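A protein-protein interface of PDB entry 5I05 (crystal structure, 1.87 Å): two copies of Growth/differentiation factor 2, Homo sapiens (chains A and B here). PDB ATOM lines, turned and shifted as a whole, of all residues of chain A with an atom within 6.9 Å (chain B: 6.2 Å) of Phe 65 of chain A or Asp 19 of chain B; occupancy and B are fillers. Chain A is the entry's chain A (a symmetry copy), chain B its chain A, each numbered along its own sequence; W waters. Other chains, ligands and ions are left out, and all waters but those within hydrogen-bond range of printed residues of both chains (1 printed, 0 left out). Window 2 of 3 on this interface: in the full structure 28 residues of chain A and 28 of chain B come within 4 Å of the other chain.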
ATOM      1  N   LEU A  60      -5.899 -30.847 -17.671  1.00  0.00           N
ATOM      2  CA  LEU A  60      -7.260 -30.329 -17.517  1.00  0.00           C
ATOM      3  C   LEU A  60      -7.313 -28.811 -17.667  1.00  0.00           C
ATOM      4  O   LEU A  60      -8.247 -28.268 -18.284  1.00  0.00           O
ATOM      5  CB  LEU A  60      -7.827 -30.741 -16.159  1.00  0.00           C
ATOM      6  CG  LEU A  60      -7.944 -32.255 -15.990  1.00  0.00           C
ATOM      7  CD1 LEU A  60      -8.169 -32.601 -14.530  1.00  0.00           C
ATOM      8  CD2 LEU A  60      -9.102 -32.766 -16.839  1.00  0.00           C
ATOM      9  N   VAL A  61      -6.343 -28.099 -17.076  1.00  0.00           N
ATOM     10  CA  VAL A  61      -6.330 -26.643 -17.203  1.00  0.00           C
ATOM     11  C   VAL A  61      -6.162 -26.242 -18.665  1.00  0.00           C
ATOM     12  O   VAL A  61      -6.806 -25.295 -19.142  1.00  0.00           O
ATOM     13  CB  VAL A  61      -5.224 -26.024 -16.325  1.00  0.00           C
ATOM     14  CG1 VAL A  61      -5.161 -24.519 -16.538  1.00  0.00           C
ATOM     15  CG2 VAL A  61      -5.472 -26.321 -14.850  1.00  0.00           C
ATOM     16  N   HIS A  62      -5.274 -26.932 -19.385  1.00  0.00           N
ATOM     17  CA  HIS A  62      -5.074 -26.651 -20.803  1.00  0.00           C
ATOM     18  C   HIS A  62      -6.364 -26.847 -21.582  1.00  0.00           C
ATOM     19  O   HIS A  62      -6.714 -26.022 -22.434  1.00  0.00           O
ATOM     20  CB  HIS A  62      -3.984 -27.548 -21.382  1.00  0.00           C
ATOM     21  CG  HIS A  62      -3.917 -27.506 -22.878  1.00  0.00           C
ATOM     22  ND1 HIS A  62      -3.308 -26.477 -23.564  1.00  0.00           N
ATOM     23  CD2 HIS A  62      -4.424 -28.338 -23.821  1.00  0.00           C
ATOM     24  CE1 HIS A  62      -3.409 -26.694 -24.864  1.00  0.00           C
ATOM     25  NE2 HIS A  62      -4.086 -27.815 -25.047  1.00  0.00           N
ATOM     26  N   LEU A  63      -7.088 -27.936 -21.305  1.00  0.00           N
ATOM     27  CA  LEU A  63      -8.409 -28.109 -21.908  1.00  0.00           C
ATOM     28  C   LEU A  63      -9.282 -26.880 -21.696  1.00  0.00           C
ATOM     29  O   LEU A  63      -9.871 -26.351 -22.648  1.00  0.00           O
ATOM     30  CB  LEU A  63      -9.112 -29.336 -21.326  1.00  0.00           C
ATOM     31  CG  LEU A  63      -8.971 -30.620 -22.129  1.00  0.00           C
ATOM     32  CD1 LEU A  63      -7.534 -31.081 -22.179  1.00  0.00           C
ATOM     33  CD2 LEU A  63      -9.863 -31.690 -21.539  1.00  0.00           C
ATOM     34  N   LYS A  64      -9.395 -26.421 -20.445  1.00  0.00           N
ATOM     35  CA  LYS A  64     -10.253 -25.269 -20.168  1.00  0.00           C
ATOM     36  C   LYS A  64      -9.732 -23.992 -20.826  1.00  0.00           C
ATOM     37  O   LYS A  64     -10.521 -23.186 -21.334  1.00  0.00           O
ATOM     38  CB  LYS A  64     -10.393 -25.061 -18.657  1.00  0.00           C
ATOM     39  CG  LYS A  64     -11.343 -26.019 -17.963  1.00  0.00           C
ATOM     40  CD  LYS A  64     -12.801 -25.730 -18.292  1.00  0.00           C
ATOM     41  CE  LYS A  64     -13.317 -24.452 -17.643  1.00  0.00           C
ATOM     42  NZ  LYS A  64     -14.751 -24.191 -18.007  1.00  0.00           N
ATOM     43  N   PHE A  65      -8.415 -23.773 -20.806  1.00  0.00           N
ATOM     44  CA  PHE A  65      -7.806 -22.522 -21.271  1.00  0.00           C
ATOM     45  C   PHE A  65      -6.653 -22.837 -22.216  1.00  0.00           C
ATOM     46  O   PHE A  65      -5.478 -22.599 -21.894  1.00  0.00           O
ATOM     47  CB  PHE A  65      -7.309 -21.671 -20.098  1.00  0.00           C
ATOM     48  CG  PHE A  65      -8.319 -21.484 -19.001  1.00  0.00           C
ATOM     49  CD1 PHE A  65      -8.377 -22.368 -17.942  1.00  0.00           C
ATOM     50  CD2 PHE A  65      -9.195 -20.413 -19.020  1.00  0.00           C
ATOM     51  CE1 PHE A  65      -9.296 -22.195 -16.923  1.00  0.00           C
ATOM     52  CE2 PHE A  65     -10.118 -20.237 -18.003  1.00  0.00           C
ATOM     53  CZ  PHE A  65     -10.167 -21.130 -16.955  1.00  0.00           C
ATOM     54  N   PRO A  66      -6.952 -23.341 -23.416  1.00  0.00           N
ATOM     55  CA  PRO A  66      -5.870 -23.828 -24.287  1.00  0.00           C
ATOM     56  C   PRO A  66      -4.883 -22.758 -24.730  1.00  0.00           C
ATOM     57  O   PRO A  66      -3.737 -23.099 -25.045  1.00  0.00           O
ATOM     58  CB  PRO A  66      -6.622 -24.424 -25.488  1.00  0.00           C
ATOM     59  CG  PRO A  66      -8.000 -23.841 -25.430  1.00  0.00           C
ATOM     60  CD  PRO A  66      -8.282 -23.630 -23.969  1.00  0.00           C
ATOM     61  N   THR A  67      -5.282 -21.483 -24.790  1.00  0.00           N
ATOM     62  CA  THR A  67      -4.358 -20.452 -25.264  1.00  0.00           C
ATOM     63  C   THR A  67      -3.461 -19.920 -24.155  1.00  0.00           C
ATOM     64  O   THR A  67      -2.354 -19.445 -24.436  1.00  0.00           O
ATOM     65  CB  THR A  67      -5.124 -19.282 -25.885  1.00  0.00           C
ATOM     66  OG1 THR A  67      -5.970 -18.687 -24.892  1.00  0.00           O
ATOM     67  CG2 THR A  67      -5.973 -19.755 -27.061  1.00  0.00           C
ATOM     68  N   LYS A  68      -3.913 -19.982 -22.904  1.00  0.00           N
ATOM     69  CA  LYS A  68      -3.136 -19.466 -21.787  1.00  0.00           C
ATOM     70  C   LYS A  68      -2.205 -20.503 -21.165  1.00  0.00           C
ATOM     71  O   LYS A  68      -1.182 -20.129 -20.584  1.00  0.00           O
ATOM     72  CB  LYS A  68      -4.077 -18.924 -20.706  1.00  0.00           C
ATOM     73  CG  LYS A  68      -5.108 -17.923 -21.219  1.00  0.00           C
ATOM     74  CD  LYS A  68      -5.909 -17.304 -20.077  1.00  0.00           C
ATOM     75  CE  LYS A  68      -7.114 -16.534 -20.597  1.00  0.00           C
ATOM     76  NZ  LYS A  68      -6.760 -15.607 -21.711  1.00  0.00           N
ATOM     77  N   VAL A  69      -2.530 -21.791 -21.259  1.00  0.00           N
ATOM     78  CA  VAL A  69      -1.805 -22.838 -20.546  1.00  0.00           C
ATOM     79  C   VAL A  69      -1.519 -23.990 -21.500  1.00  0.00           C
ATOM     80  O   VAL A  69      -2.440 -24.528 -22.123  1.00  0.00           O
ATOM     81  CB  VAL A  69      -2.598 -23.345 -19.324  1.00  0.00           C
ATOM     82  CG1 VAL A  69      -1.858 -24.501 -18.645  1.00  0.00           C
ATOM     83  CG2 VAL A  69      -2.839 -22.218 -18.342  1.00  0.00           C
ATOM     84  N   GLY A  70      -0.249 -24.400 -21.573  1.00  0.00           N
ATOM     85  CA  GLY A  70       0.145 -25.495 -22.436  1.00  0.00           C
ATOM     86  C   GLY A  70      -0.138 -26.866 -21.835  1.00  0.00           C
ATOM     87  O   GLY A  70      -0.477 -27.017 -20.661  1.00  0.00           O
ATOM     88  N   VAL B  15      -4.712 -22.671 -10.114  1.00  0.00           N
ATOM     89  CA  VAL B  15      -5.651 -23.713 -10.522  1.00  0.00           C
ATOM     90  C   VAL B  15      -6.899 -23.662  -9.645  1.00  0.00           C
ATOM     91  O   VAL B  15      -6.807 -23.739  -8.413  1.00  0.00           O
ATOM     92  CB  VAL B  15      -5.012 -25.108 -10.441  1.00  0.00           C
ATOM     93  CG1 VAL B  15      -6.011 -26.171 -10.880  1.00  0.00           C
ATOM     94  CG2 VAL B  15      -3.748 -25.165 -11.297  1.00  0.00           C
ATOM     95  N   ASN B  16      -8.064 -23.598 -10.292  1.00  0.00           N
ATOM     96  CA  ASN B  16      -9.365 -23.673  -9.631  1.00  0.00           C
ATOM     97  C   ASN B  16      -9.928 -25.078  -9.811  1.00  0.00           C
ATOM     98  O   ASN B  16     -10.092 -25.552 -10.945  1.00  0.00           O
ATOM     99  CB  ASN B  16     -10.325 -22.633 -10.210  1.00  0.00           C
ATOM    100  CG  ASN B  16     -11.692 -22.681  -9.569  1.00  0.00           C
ATOM    101  OD1 ASN B  16     -12.424 -23.663  -9.713  1.00  0.00           O
ATOM    102  ND2 ASN B  16     -12.049 -21.617  -8.859  1.00  0.00           N
ATOM    103  N   PHE B  17     -10.228 -25.742  -8.697  1.00  0.00           N
ATOM    104  CA  PHE B  17     -10.615 -27.143  -8.773  1.00  0.00           C
ATOM    105  C   PHE B  17     -11.969 -27.329  -9.439  1.00  0.00           C
ATOM    106  O   PHE B  17     -12.210 -28.391 -10.028  1.00  0.00           O
ATOM    107  CB  PHE B  17     -10.611 -27.774  -7.379  1.00  0.00           C
ATOM    108  CG  PHE B  17      -9.225 -28.040  -6.840  1.00  0.00           C
ATOM    109  CD1 PHE B  17      -8.367 -28.911  -7.499  1.00  0.00           C
ATOM    110  CD2 PHE B  17      -8.784 -27.426  -5.682  1.00  0.00           C
ATOM    111  CE1 PHE B  17      -7.090 -29.156  -7.017  1.00  0.00           C
ATOM    112  CE2 PHE B  17      -7.506 -27.668  -5.187  1.00  0.00           C
ATOM    113  CZ  PHE B  17      -6.660 -28.537  -5.854  1.00  0.00           C
ATOM    114  N   GLU B  18     -12.843 -26.320  -9.388  1.00  0.00           N
ATOM    115  CA  GLU B  18     -14.110 -26.409 -10.110  1.00  0.00           C
ATOM    116  C   GLU B  18     -13.871 -26.398 -11.610  1.00  0.00           C
ATOM    117  O   GLU B  18     -14.481 -27.184 -12.346  1.00  0.00           O
ATOM    118  CB  GLU B  18     -15.035 -25.255  -9.716  1.00  0.00           C
ATOM    119  CG  GLU B  18     -16.447 -25.367 -10.315  1.00  0.00           C
ATOM    120  CD  GLU B  18     -17.341 -24.178  -9.972  1.00  0.00           C
ATOM    121  OE1 GLU B  18     -17.027 -23.453  -9.008  1.00  0.00           O
ATOM    122  OE2 GLU B  18     -18.359 -23.966 -10.669  1.00  0.00           O
ATOM    123  N   ASP B  19     -12.971 -25.522 -12.075  1.00  0.00           N
ATOM    124  CA  ASP B  19     -12.628 -25.451 -13.495  1.00  0.00           C
ATOM    125  C   ASP B  19     -12.217 -26.805 -14.055  1.00  0.00           C
ATOM    126  O   ASP B  19     -12.442 -27.083 -15.240  1.00  0.00           O
ATOM    127  CB  ASP B  19     -11.483 -24.459 -13.728  1.00  0.00           C
ATOM    128  CG  ASP B  19     -11.896 -23.020 -13.559  1.00  0.00           C
ATOM    129  OD1 ASP B  19     -13.107 -22.747 -13.450  1.00  0.00           O
ATOM    130  OD2 ASP B  19     -10.989 -22.153 -13.547  1.00  0.00           O
ATOM    131  N   ILE B  20     -11.539 -27.629 -13.252  1.00  0.00           N
ATOM    132  CA  ILE B  20     -11.024 -28.914 -13.730  1.00  0.00           C
ATOM    133  C   ILE B  20     -11.899 -30.081 -13.288  1.00  0.00           C
ATOM    134  O   ILE B  20     -11.504 -31.239 -13.457  1.00  0.00           O
ATOM    135  CB  ILE B  20      -9.569 -29.145 -13.290  1.00  0.00           C
ATOM    136  CG1 ILE B  20      -9.449 -29.270 -11.765  1.00  0.00           C
ATOM    137  CG2 ILE B  20      -8.684 -28.026 -13.795  1.00  0.00           C
ATOM    138  CD1 ILE B  20      -8.120 -29.857 -11.311  1.00  0.00           C
ATOM    139  N   GLY B  21     -13.072 -29.806 -12.720  1.00  0.00           N
ATOM    140  CA  GLY B  21     -14.000 -30.852 -12.334  1.00  0.00           C
ATOM    141  C   GLY B  21     -13.628 -31.643 -11.100  1.00  0.00           C
ATOM    142  O   GLY B  21     -14.197 -32.716 -10.874  1.00  0.00           O
ATOM    143  N   TRP B  22     -12.711 -31.143 -10.277  1.00  0.00           N
ATOM    144  CA  TRP B  22     -12.333 -31.833  -9.053  1.00  0.00           C
ATOM    145  C   TRP B  22     -13.097 -31.340  -7.827  1.00  0.00           C
ATOM    146  O   TRP B  22     -13.010 -31.972  -6.766  1.00  0.00           O
ATOM    147  CB  TRP B  22     -10.822 -31.688  -8.820  1.00  0.00           C
ATOM    148  CG  TRP B  22     -10.001 -32.645  -9.638  1.00  0.00           C
ATOM    149  CD1 TRP B  22     -10.426 -33.388 -10.706  1.00  0.00           C
ATOM    150  CD2 TRP B  22      -8.614 -32.965  -9.458  1.00  0.00           C
ATOM    151  NE1 TRP B  22      -9.388 -34.150 -11.197  1.00  0.00           N
ATOM    152  CE2 TRP B  22      -8.270 -33.910 -10.444  1.00  0.00           C
ATOM    153  CE3 TRP B  22      -7.635 -32.555  -8.548  1.00  0.00           C
ATOM    154  CZ2 TRP B  22      -6.988 -34.442 -10.550  1.00  0.00           C
ATOM    155  CZ3 TRP B  22      -6.361 -33.089  -8.661  1.00  0.00           C
ATOM    156  CH2 TRP B  22      -6.055 -34.021  -9.654  1.00  0.00           C
ATOM    157  N   ASP B  23     -13.849 -30.243  -7.952  1.00  0.00           N
ATOM    158  CA  ASP B  23     -14.639 -29.724  -6.841  1.00  0.00           C
ATOM    159  C   ASP B  23     -15.640 -30.742  -6.308  1.00  0.00           C
ATOM    160  O   ASP B  23     -16.149 -30.570  -5.196  1.00  0.00           O
ATOM    161  CB  ASP B  23     -15.390 -28.467  -7.278  1.00  0.00           C
ATOM    162  CG  ASP B  23     -16.402 -28.754  -8.364  1.00  0.00           C
ATOM    163  OD1 ASP B  23     -16.205 -29.747  -9.098  1.00  0.00           O
ATOM    164  OD2 ASP B  23     -17.382 -27.992  -8.489  1.00  0.00           O
ATOM    165  N   GLU B  31      -8.903 -22.896  -4.761  1.00  0.00           N
ATOM    166  CA  GLU B  31      -7.836 -22.755  -5.743  1.00  0.00           C
ATOM    167  C   GLU B  31      -6.494 -22.987  -5.061  1.00  0.00           C
ATOM    168  O   GLU B  31      -6.377 -22.914  -3.836  1.00  0.00           O
ATOM    169  CB  GLU B  31      -7.847 -21.364  -6.384  1.00  0.00           C
ATOM    170  CG  GLU B  31      -9.155 -20.983  -7.045  1.00  0.00           C
ATOM    171  CD  GLU B  31      -9.124 -19.588  -7.632  1.00  0.00           C
ATOM    172  OE1 GLU B  31      -8.205 -18.816  -7.287  1.00  0.00           O
ATOM    173  OE2 GLU B  31     -10.015 -19.265  -8.443  1.00  0.00           O
HETATM  174  O   HOH W   1     -15.024 -26.897 -16.092  1.00  0.00           O
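No position is printed for both chains. Of the 5 pairs that touch across the chains among the printed residues, none has its exchanged pair printed and touching as well.
Among the printed residues, pairs that only touch across the chains: Leu 60 of chain A with Ile 20 of chain B, Leu 60 of chain A with Trp 22 of chain B, Val 61 of chain A with Ile 20 of chain B, Lys 64 of chain A with Asp 19 of chain B and Phe 65 of chain A with Asp 19 of chain B.
The backbone NH (N) of Trp 22 of chain B is in hydrogen-bond range of the backbone carbonyl oxygen (O) of Phe 17 of chain B. The backbone NH of Asp 19 of chain B sits at hydrogen-bond distance from the side-chain amide oxygen of Asn 16 of chain B (3.1 Å).
Of the printed residues of chain B, Lys 64 of chain A touches Asp 19 (3.1 Å). Phe 65 of chain A touches just one residue of chain B: Asp 19. Thr 67 of chain A touches none of the printed residues of chain B. Gly 70 of chain A touches none of the printed residues of chain B. Of chain A, only Lys 64 (3.1 Å) and Phe 65 (3.7 Å) come within 4 Å of Asp 19 of chain B. Of the printed residues of chain A, Ile 20 of chain B touches Leu 60 and Val 61. Of the printed residues of chain A, Trp 22 of chain B touches Leu 60 (3.9 Å).
Water W1 bridges the backbone carbonyl oxygen (O) of Asp 19 of chain B (2.7 Å) and the side-chain amino group (NZ) of Lys 64 of chain A (3.3 Å).
Printed residues of chain A that touch a printed residue of chain B: Leu 60, Val 61, Lys 64 and Phe 65. Hydrophobic or aromatic side chains of chain A that line the printed part of chain B: Leu 60, Val 61 and Phe 65. Printed residues of chain B that touch a printed residue of chain A: Asp 19, Ile 20 and Trp 22. Among the printed residues, no Asp or Glu carboxylate lies within 4 Å of a Lys or Arg side-chain nitrogen of the other chain.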
